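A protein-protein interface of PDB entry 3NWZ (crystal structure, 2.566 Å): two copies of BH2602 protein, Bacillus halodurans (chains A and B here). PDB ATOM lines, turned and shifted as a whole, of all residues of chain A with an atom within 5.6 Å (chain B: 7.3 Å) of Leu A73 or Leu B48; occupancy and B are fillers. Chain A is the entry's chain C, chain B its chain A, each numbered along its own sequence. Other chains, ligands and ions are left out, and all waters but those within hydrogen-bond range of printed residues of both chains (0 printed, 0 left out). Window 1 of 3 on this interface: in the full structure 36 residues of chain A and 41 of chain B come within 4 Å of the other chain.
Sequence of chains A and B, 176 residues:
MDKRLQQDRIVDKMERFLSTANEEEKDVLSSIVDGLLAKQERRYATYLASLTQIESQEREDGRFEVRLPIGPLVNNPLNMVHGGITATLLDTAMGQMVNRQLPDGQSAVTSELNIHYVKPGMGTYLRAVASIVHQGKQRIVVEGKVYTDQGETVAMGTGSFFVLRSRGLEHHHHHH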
ATOM      1  N   VAL A  28      -9.260   5.889  31.088  1.00  0.00           N
ATOM      2  CA  VAL A  28      -8.452   4.984  30.276  1.00  0.00           C
ATOM      3  C   VAL A  28      -8.045   3.819  31.157  1.00  0.00           C
ATOM      4  O   VAL A  28      -8.045   2.664  30.728  1.00  0.00           O
ATOM      5  CB  VAL A  28      -7.174   5.688  29.732  1.00  0.00           C
ATOM      6  CG1 VAL A  28      -6.026   4.694  29.610  1.00  0.00           C
ATOM      7  CG2 VAL A  28      -7.471   6.310  28.380  1.00  0.00           C
ATOM      8  N   ILE A  32      -9.045  -0.192  30.894  1.00  0.00           N
ATOM      9  CA  ILE A  32      -7.986  -1.192  30.837  1.00  0.00           C
ATOM     10  C   ILE A  32      -8.269  -2.306  31.836  1.00  0.00           C
ATOM     11  O   ILE A  32      -8.203  -3.485  31.488  1.00  0.00           O
ATOM     12  CB  ILE A  32      -6.586  -0.551  31.080  1.00  0.00           C
ATOM     13  CG1 ILE A  32      -6.113   0.120  29.782  1.00  0.00           C
ATOM     14  CG2 ILE A  32      -5.544  -1.625  31.548  1.00  0.00           C
ATOM     15  CD1 ILE A  32      -4.770   0.803  29.893  1.00  0.00           C
ATOM     16  N   LEU A  51      -7.456  -4.781  26.169  1.00  0.00           N
ATOM     17  CA  LEU A  51      -7.362  -3.337  26.222  1.00  0.00           C
ATOM     18  C   LEU A  51      -7.964  -2.629  25.028  1.00  0.00           C
ATOM     19  O   LEU A  51      -8.502  -1.533  25.166  1.00  0.00           O
ATOM     20  CB  LEU A  51      -5.903  -2.926  26.413  1.00  0.00           C
ATOM     21  CG  LEU A  51      -5.332  -3.374  27.763  1.00  0.00           C
ATOM     22  CD1 LEU A  51      -5.391  -4.880  27.868  1.00  0.00           C
ATOM     23  CD2 LEU A  51      -3.902  -2.902  27.916  1.00  0.00           C
ATOM     24  N   THR A  52      -7.890  -3.244  23.855  1.00  0.00           N
ATOM     25  CA  THR A  52      -8.450  -2.610  22.666  1.00  0.00           C
ATOM     26  C   THR A  52      -9.972  -2.602  22.724  1.00  0.00           C
ATOM     27  O   THR A  52     -10.602  -1.614  22.337  1.00  0.00           O
ATOM     28  CB  THR A  52      -8.017  -3.319  21.384  1.00  0.00           C
ATOM     29  OG1 THR A  52      -8.697  -2.731  20.273  1.00  0.00           O
ATOM     30  CG2 THR A  52      -8.363  -4.783  21.439  1.00  0.00           C
ATOM     31  N   GLY A  71     -11.018   5.125  21.479  1.00  0.00           N
ATOM     32  CA  GLY A  71     -10.707   5.908  22.664  1.00  0.00           C
ATOM     33  C   GLY A  71      -9.274   6.441  22.627  1.00  0.00           C
ATOM     34  O   GLY A  71      -8.606   6.336  21.593  1.00  0.00           O
ATOM     35  N   PRO A  72      -8.778   7.041  23.727  1.00  0.00           N
ATOM     36  CA  PRO A  72      -7.407   7.569  23.756  1.00  0.00           C
ATOM     37  C   PRO A  72      -6.339   6.468  23.750  1.00  0.00           C
ATOM     38  O   PRO A  72      -5.189   6.694  23.378  1.00  0.00           O
ATOM     39  CB  PRO A  72      -7.386   8.400  25.038  1.00  0.00           C
ATOM     40  CG  PRO A  72      -8.809   8.891  25.132  1.00  0.00           C
ATOM     41  CD  PRO A  72      -9.565   7.609  24.835  1.00  0.00           C
ATOM     42  N   LEU A  73      -6.719   5.271  24.163  1.00  0.00           N
ATOM     43  CA  LEU A  73      -5.782   4.160  24.173  1.00  0.00           C
ATOM     44  C   LEU A  73      -5.422   3.724  22.737  1.00  0.00           C
ATOM     45  O   LEU A  73      -4.514   2.914  22.537  1.00  0.00           O
ATOM     46  CB  LEU A  73      -6.409   2.989  24.923  1.00  0.00           C
ATOM     47  CG  LEU A  73      -5.617   1.694  25.041  1.00  0.00           C
ATOM     48  CD1 LEU A  73      -4.556   1.816  26.129  1.00  0.00           C
ATOM     49  CD2 LEU A  73      -6.579   0.568  25.376  1.00  0.00           C
ATOM     50  N   VAL A  74      -6.112   4.273  21.740  1.00  0.00           N
ATOM     51  CA  VAL A  74      -5.876   3.878  20.349  1.00  0.00           C
ATOM     52  C   VAL A  74      -5.473   4.996  19.381  1.00  0.00           C
ATOM     53  O   VAL A  74      -5.066   4.728  18.249  1.00  0.00           O
ATOM     54  CB  VAL A  74      -7.133   3.171  19.786  1.00  0.00           C
ATOM     55  CG1 VAL A  74      -6.895   2.714  18.368  1.00  0.00           C
ATOM     56  CG2 VAL A  74      -7.487   1.981  20.657  1.00  0.00           C
ATOM     57  N   ASN A  75      -5.573   6.244  19.823  1.00  0.00           N
ATOM     58  CA  ASN A  75      -5.244   7.386  18.977  1.00  0.00           C
ATOM     59  C   ASN A  75      -3.765   7.761  18.947  1.00  0.00           C
ATOM     60  O   ASN A  75      -2.978   7.303  19.770  1.00  0.00           O
ATOM     61  CB  ASN A  75      -6.061   8.594  19.421  1.00  0.00           C
ATOM     62  CG  ASN A  75      -7.553   8.362  19.299  1.00  0.00           C
ATOM     63  OD1 ASN A  75      -8.354   9.199  19.711  1.00  0.00           O
ATOM     64  ND2 ASN A  75      -7.934   7.223  18.727  1.00  0.00           N
ATOM     65  N   ILE A  85      -2.907   0.464  14.596  1.00  0.00           N
ATOM     66  CA  ILE A  85      -4.089  -0.203  15.141  1.00  0.00           C
ATOM     67  C   ILE A  85      -5.145  -0.488  14.076  1.00  0.00           C
ATOM     68  O   ILE A  85      -5.806  -1.523  14.125  1.00  0.00           O
ATOM     69  CB  ILE A  85      -4.784   0.631  16.255  1.00  0.00           C
ATOM     70  CG1 ILE A  85      -3.845   0.834  17.447  1.00  0.00           C
ATOM     71  CG2 ILE A  85      -6.054  -0.084  16.697  1.00  0.00           C
ATOM     72  CD1 ILE A  85      -3.421  -0.448  18.131  1.00  0.00           C
ATOM     73  N   ILE B  32       1.558  -2.109  32.750  1.00  0.00           N
ATOM     74  CA  ILE B  32       0.518  -1.182  32.338  1.00  0.00           C
ATOM     75  C   ILE B  32       0.473   0.017  33.265  1.00  0.00           C
ATOM     76  O   ILE B  32       0.522   1.150  32.797  1.00  0.00           O
ATOM     77  CB  ILE B  32      -0.866  -1.861  32.299  1.00  0.00           C
ATOM     78  CG1 ILE B  32      -0.935  -2.787  31.083  1.00  0.00           C
ATOM     79  CG2 ILE B  32      -1.967  -0.814  32.244  1.00  0.00           C
ATOM     80  CD1 ILE B  32      -2.282  -3.424  30.862  1.00  0.00           C
ATOM     81  N   LEU B  36       0.974   3.991  31.921  1.00  0.00           N
ATOM     82  CA  LEU B  36       0.034   5.078  32.210  1.00  0.00           C
ATOM     83  C   LEU B  36       0.673   6.145  33.092  1.00  0.00           C
ATOM     84  O   LEU B  36       0.398   7.326  32.960  1.00  0.00           O
ATOM     85  CB  LEU B  36      -1.195   4.513  32.926  1.00  0.00           C
ATOM     86  CG  LEU B  36      -1.849   3.243  32.358  1.00  0.00           C
ATOM     87  CD1 LEU B  36      -2.997   2.816  33.268  1.00  0.00           C
ATOM     88  CD2 LEU B  36      -2.353   3.497  30.943  1.00  0.00           C
ATOM     89  N   LYS B  39       3.034   7.938  31.209  1.00  0.00           N
ATOM     90  CA  LYS B  39       2.227   8.694  30.267  1.00  0.00           C
ATOM     91  C   LYS B  39       1.927  10.072  30.839  1.00  0.00           C
ATOM     92  O   LYS B  39       2.207  11.075  30.185  1.00  0.00           O
ATOM     93  CB  LYS B  39       0.913   7.966  29.951  1.00  0.00           C
ATOM     94  CG  LYS B  39      -0.072   8.742  29.040  1.00  0.00           C
ATOM     95  CD  LYS B  39       0.521   9.085  27.674  1.00  0.00           C
ATOM     96  CE  LYS B  39      -0.513   9.742  26.755  1.00  0.00           C
ATOM     97  NZ  LYS B  39      -1.017  11.032  27.307  1.00  0.00           N
ATOM     98  N   TYR B  44       6.141  10.225  27.293  1.00  0.00           N
ATOM     99  CA  TYR B  44       5.591   9.644  26.055  1.00  0.00           C
ATOM    100  C   TYR B  44       4.345  10.435  25.624  1.00  0.00           C
ATOM    101  O   TYR B  44       3.466  10.718  26.437  1.00  0.00           O
ATOM    102  CB  TYR B  44       5.152   8.196  26.276  1.00  0.00           C
ATOM    103  CG  TYR B  44       6.255   7.192  26.357  1.00  0.00           C
ATOM    104  CD1 TYR B  44       7.031   6.900  25.243  1.00  0.00           C
ATOM    105  CD2 TYR B  44       6.515   6.509  27.540  1.00  0.00           C
ATOM    106  CE1 TYR B  44       8.043   5.946  25.299  1.00  0.00           C
ATOM    107  CE2 TYR B  44       7.526   5.549  27.608  1.00  0.00           C
ATOM    108  CZ  TYR B  44       8.285   5.275  26.480  1.00  0.00           C
ATOM    109  OH  TYR B  44       9.279   4.332  26.519  1.00  0.00           O
ATOM    110  N   ALA B  45       4.247  10.766  24.344  1.00  0.00           N
ATOM    111  CA  ALA B  45       3.083  11.512  23.858  1.00  0.00           C
ATOM    112  C   ALA B  45       1.811  10.671  23.887  1.00  0.00           C
ATOM    113  O   ALA B  45       0.744  11.185  24.227  1.00  0.00           O
ATOM    114  CB  ALA B  45       3.320  12.033  22.419  1.00  0.00           C
ATOM    115  N   THR B  46       1.935   9.387  23.542  1.00  0.00           N
ATOM    116  CA  THR B  46       0.793   8.472  23.473  1.00  0.00           C
ATOM    117  C   THR B  46       0.838   7.266  24.411  1.00  0.00           C
ATOM    118  O   THR B  46       1.898   6.858  24.900  1.00  0.00           O
ATOM    119  CB  THR B  46       0.640   7.892  22.065  1.00  0.00           C
ATOM    120  OG1 THR B  46       1.750   7.017  21.799  1.00  0.00           O
ATOM    121  CG2 THR B  46       0.600   8.991  21.038  1.00  0.00           C
ATOM    122  N   TYR B  47      -0.337   6.677  24.613  1.00  0.00           N
ATOM    123  CA  TYR B  47      -0.486   5.511  25.473  1.00  0.00           C
ATOM    124  C   TYR B  47       0.142   4.281  24.842  1.00  0.00           C
ATOM    125  O   TYR B  47       0.748   3.459  25.534  1.00  0.00           O
ATOM    126  CB  TYR B  47      -1.970   5.231  25.739  1.00  0.00           C
ATOM    127  CG  TYR B  47      -2.636   6.287  26.571  1.00  0.00           C
ATOM    128  CD1 TYR B  47      -3.244   7.384  25.975  1.00  0.00           C
ATOM    129  CD2 TYR B  47      -2.604   6.224  27.963  1.00  0.00           C
ATOM    130  CE1 TYR B  47      -3.800   8.401  26.745  1.00  0.00           C
ATOM    131  CE2 TYR B  47      -3.152   7.231  28.734  1.00  0.00           C
ATOM    132  CZ  TYR B  47      -3.744   8.320  28.122  1.00  0.00           C
ATOM    133  OH  TYR B  47      -4.236   9.356  28.883  1.00  0.00           O
ATOM    134  N   LEU B  48      -0.008   4.154  23.529  1.00  0.00           N
ATOM    135  CA  LEU B  48       0.535   3.006  22.817  1.00  0.00           C
ATOM    136  C   LEU B  48       2.047   2.892  22.986  1.00  0.00           C
ATOM    137  O   LEU B  48       2.552   1.831  23.338  1.00  0.00           O
ATOM    138  CB  LEU B  48       0.165   3.091  21.338  1.00  0.00           C
ATOM    139  CG  LEU B  48      -0.487   1.806  20.812  1.00  0.00           C
ATOM    140  CD1 LEU B  48       0.562   0.705  20.603  1.00  0.00           C
ATOM    141  CD2 LEU B  48      -1.568   1.349  21.795  1.00  0.00           C
ATOM    142  N   ALA B  49       2.751   3.995  22.738  1.00  0.00           N
ATOM    143  CA  ALA B  49       4.201   4.058  22.872  1.00  0.00           C
ATOM    144  C   ALA B  49       4.547   3.822  24.335  1.00  0.00           C
ATOM    145  O   ALA B  49       5.416   3.015  24.664  1.00  0.00           O
ATOM    146  CB  ALA B  49       4.693   5.421  22.434  1.00  0.00           C
ATOM    147  N   SER B  50       3.845   4.534  25.212  1.00  0.00           N
ATOM    148  CA  SER B  50       4.039   4.416  26.654  1.00  0.00           C
ATOM    149  C   SER B  50       3.833   3.000  27.207  1.00  0.00           C
ATOM    150  O   SER B  50       4.621   2.531  28.032  1.00  0.00           O
ATOM    151  CB  SER B  50       3.095   5.370  27.388  1.00  0.00           C
ATOM    152  OG  SER B  50       3.128   5.112  28.782  1.00  0.00           O
ATOM    153  N   LEU B  51       2.774   2.325  26.766  1.00  0.00           N
ATOM    154  CA  LEU B  51       2.484   0.983  27.253  1.00  0.00           C
ATOM    155  C   LEU B  51       3.320  -0.063  26.562  1.00  0.00           C
ATOM    156  O   LEU B  51       3.383  -1.208  27.010  1.00  0.00           O
ATOM    157  CB  LEU B  51       1.002   0.649  27.073  1.00  0.00           C
ATOM    158  CG  LEU B  51       0.010   1.211  28.105  1.00  0.00           C
ATOM    159  CD1 LEU B  51       0.371   2.626  28.504  1.00  0.00           C
ATOM    160  CD2 LEU B  51      -1.393   1.181  27.509  1.00  0.00           C
ATOM    161  N   THR B  52       3.969   0.304  25.465  1.00  0.00           N
ATOM    162  CA  THR B  52       4.790  -0.686  24.792  1.00  0.00           C
ATOM    163  C   THR B  52       6.277  -0.461  25.059  1.00  0.00           C
ATOM    164  O   THR B  52       7.101  -1.319  24.772  1.00  0.00           O
ATOM    165  CB  THR B  52       4.516  -0.713  23.294  1.00  0.00           C
ATOM    166  OG1 THR B  52       5.138  -1.870  22.736  1.00  0.00           O
ATOM    167  CG2 THR B  52       5.053   0.530  22.623  1.00  0.00           C
ATOM    168  N   GLN B  53       6.605   0.701  25.618  1.00  0.00           N
ATOM    169  CA  GLN B  53       7.982   1.058  25.966  1.00  0.00           C
ATOM    170  C   GLN B  53       8.997   1.161  24.803  1.00  0.00           C
ATOM    171  O   GLN B  53      10.175   0.866  24.988  1.00  0.00           O
ATOM    172  CB  GLN B  53       8.521   0.055  26.999  1.00  0.00           C
ATOM    173  CG  GLN B  53       7.526  -0.389  28.061  1.00  0.00           C
ATOM    174  CD  GLN B  53       7.669  -1.871  28.417  1.00  0.00           C
ATOM    175  OE1 GLN B  53       8.756  -2.335  28.773  1.00  0.00           O
ATOM    176  NE2 GLN B  53       6.570  -2.614  28.321  1.00  0.00           N
ATOM    177  N   ILE B  54       8.578   1.588  23.619  1.00  0.00           N
ATOM    178  CA  ILE B  54       9.529   1.677  22.506  1.00  0.00           C
ATOM    179  C   ILE B  54      10.713   2.632  22.736  1.00  0.00           C
ATOM    180  O   ILE B  54      10.580   3.657  23.404  1.00  0.00           O
ATOM    181  CB  ILE B  54       8.827   2.087  21.181  1.00  0.00           C
ATOM    182  CG1 ILE B  54       8.142   3.444  21.331  1.00  0.00           C
ATOM    183  CG2 ILE B  54       7.799   1.052  20.802  1.00  0.00           C
ATOM    184  CD1 ILE B  54       7.624   4.008  20.030  1.00  0.00           C
ATOM    185  N   LEU B  68      11.324  -2.735  20.515  1.00  0.00           N
ATOM    186  CA  LEU B  68      10.188  -2.936  21.388  1.00  0.00           C
ATOM    187  C   LEU B  68      10.376  -4.181  22.217  1.00  0.00           C
ATOM    188  O   LEU B  68      10.587  -5.259  21.683  1.00  0.00           O
ATOM    189  CB  LEU B  68       8.933  -3.064  20.532  1.00  0.00           C
ATOM    190  CG  LEU B  68       7.582  -3.452  21.117  1.00  0.00           C
ATOM    191  CD1 LEU B  68       6.489  -2.776  20.299  1.00  0.00           C
ATOM    192  CD2 LEU B  68       7.419  -4.957  21.086  1.00  0.00           C
ATOM    193  N   ILE B  85       1.296  -5.773  16.308  1.00  0.00           N
ATOM    194  CA  ILE B  85       2.332  -4.964  16.947  1.00  0.00           C
ATOM    195  C   ILE B  85       3.536  -4.905  16.000  1.00  0.00           C
ATOM    196  O   ILE B  85       4.244  -3.910  15.943  1.00  0.00           O
ATOM    197  CB  ILE B  85       2.770  -5.558  18.310  1.00  0.00           C
ATOM    198  CG1 ILE B  85       1.612  -5.512  19.312  1.00  0.00           C
ATOM    199  CG2 ILE B  85       3.937  -4.773  18.874  1.00  0.00           C
ATOM    200  CD1 ILE B  85       1.210  -4.116  19.751  1.00  0.00           C
ATOM    201  N   THR B  88       2.561  -2.290  13.352  1.00  0.00           N
ATOM    202  CA  THR B  88       2.576  -0.995  14.014  1.00  0.00           C
ATOM    203  C   THR B  88       3.981  -0.496  14.325  1.00  0.00           C
ATOM    204  O   THR B  88       4.208   0.704  14.385  1.00  0.00           O
ATOM    205  CB  THR B  88       1.734  -1.066  15.295  1.00  0.00           C
ATOM    206  OG1 THR B  88       0.375  -1.327  14.924  1.00  0.00           O
ATOM    207  CG2 THR B  88       1.796   0.231  16.063  1.00  0.00           C
ATOM    208  N   THR B  92       5.835   2.660  12.763  1.00  0.00           N
ATOM    209  CA  THR B  92       6.396   3.649  13.668  1.00  0.00           C
ATOM    210  C   THR B  92       7.809   4.025  13.233  1.00  0.00           C
ATOM    211  O   THR B  92       8.158   5.205  13.184  1.00  0.00           O
ATOM    212  CB  THR B  92       6.396   3.126  15.116  1.00  0.00           C
ATOM    213  OG1 THR B  92       5.063   2.754  15.478  1.00  0.00           O
ATOM    214  CG2 THR B  92       6.810   4.193  16.056  1.00  0.00           C
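The backbone carbonyl oxygen (O) of Thr B88 sits at hydrogen-bond distance from the side-chain hydroxyl (OG1) of Thr B92 (2.5 Å).
Val A28 touches Tyr B47.
Ile A32 touches Ile B32 (CG2 to CG2, 3.7 Å).
Leu B36 touches Ile A32 (CD2 to CD1, 3.8 Å).
Ile B32 touches Leu A51 (CD1 to CD2, 3.4 Å).
Tyr B47 touches Pro A72.
Leu B48 touches Leu A73.
Leu B51 touches Leu A73 (CD2 to CD1, 3.5 Å).
Thr B88 touches Ile A85 (OG1 to N, 3.8 Å).
Of the printed residues of chain B, Ile A32 touches Ile B32 and Leu B36.
Leu A73 touches two residues of chain B.
Of the printed residues of chain B, Ile A85 touches Thr B88 (3.8 Å).
Printed residues of chain A within 4 Å of Leu B36: Ile A32.
Of chain A, only Leu A73 (3.4 Å) comes within 4 Å of Leu B48.
Ala B49 touches none of the printed residues of chain A.
Printed residues of chain A within 4 Å of Leu B51: Leu A73 (3.5 Å).
Ile B85 touches none of the printed residues of chain A.
Printed residues of chain A within 4 Å of Thr B88: Ile A85.
The nearest residue of chain A that does not touch Leu B48 is Ile A85 (4.5 Å).
The nearest printed residue of chain B that does not touch Ile A32 is Leu B51 (4.2 Å).
Printed residues of chain A that touch a printed residue of chain B: Val A28, Ile A32, Leu A51, Pro A72, Leu A73 and Ile A85.
Hydrophobic or aromatic side chains of chain A that line the printed part of chain B: Val A28, Ile A32, Leu A51, Pro A72 and Leu A73.
Of the 18 printed residues of chain B, 6 touch a printed residue of chain A.
Among the printed residues, 8 pairs touch across the chains.
Ile A32 touches its own counterpart, Ile B32.
Leu A51 touches Ile B32, but with the chains exchanged Ile A32 does not touch Leu B51 (4.2 Å).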
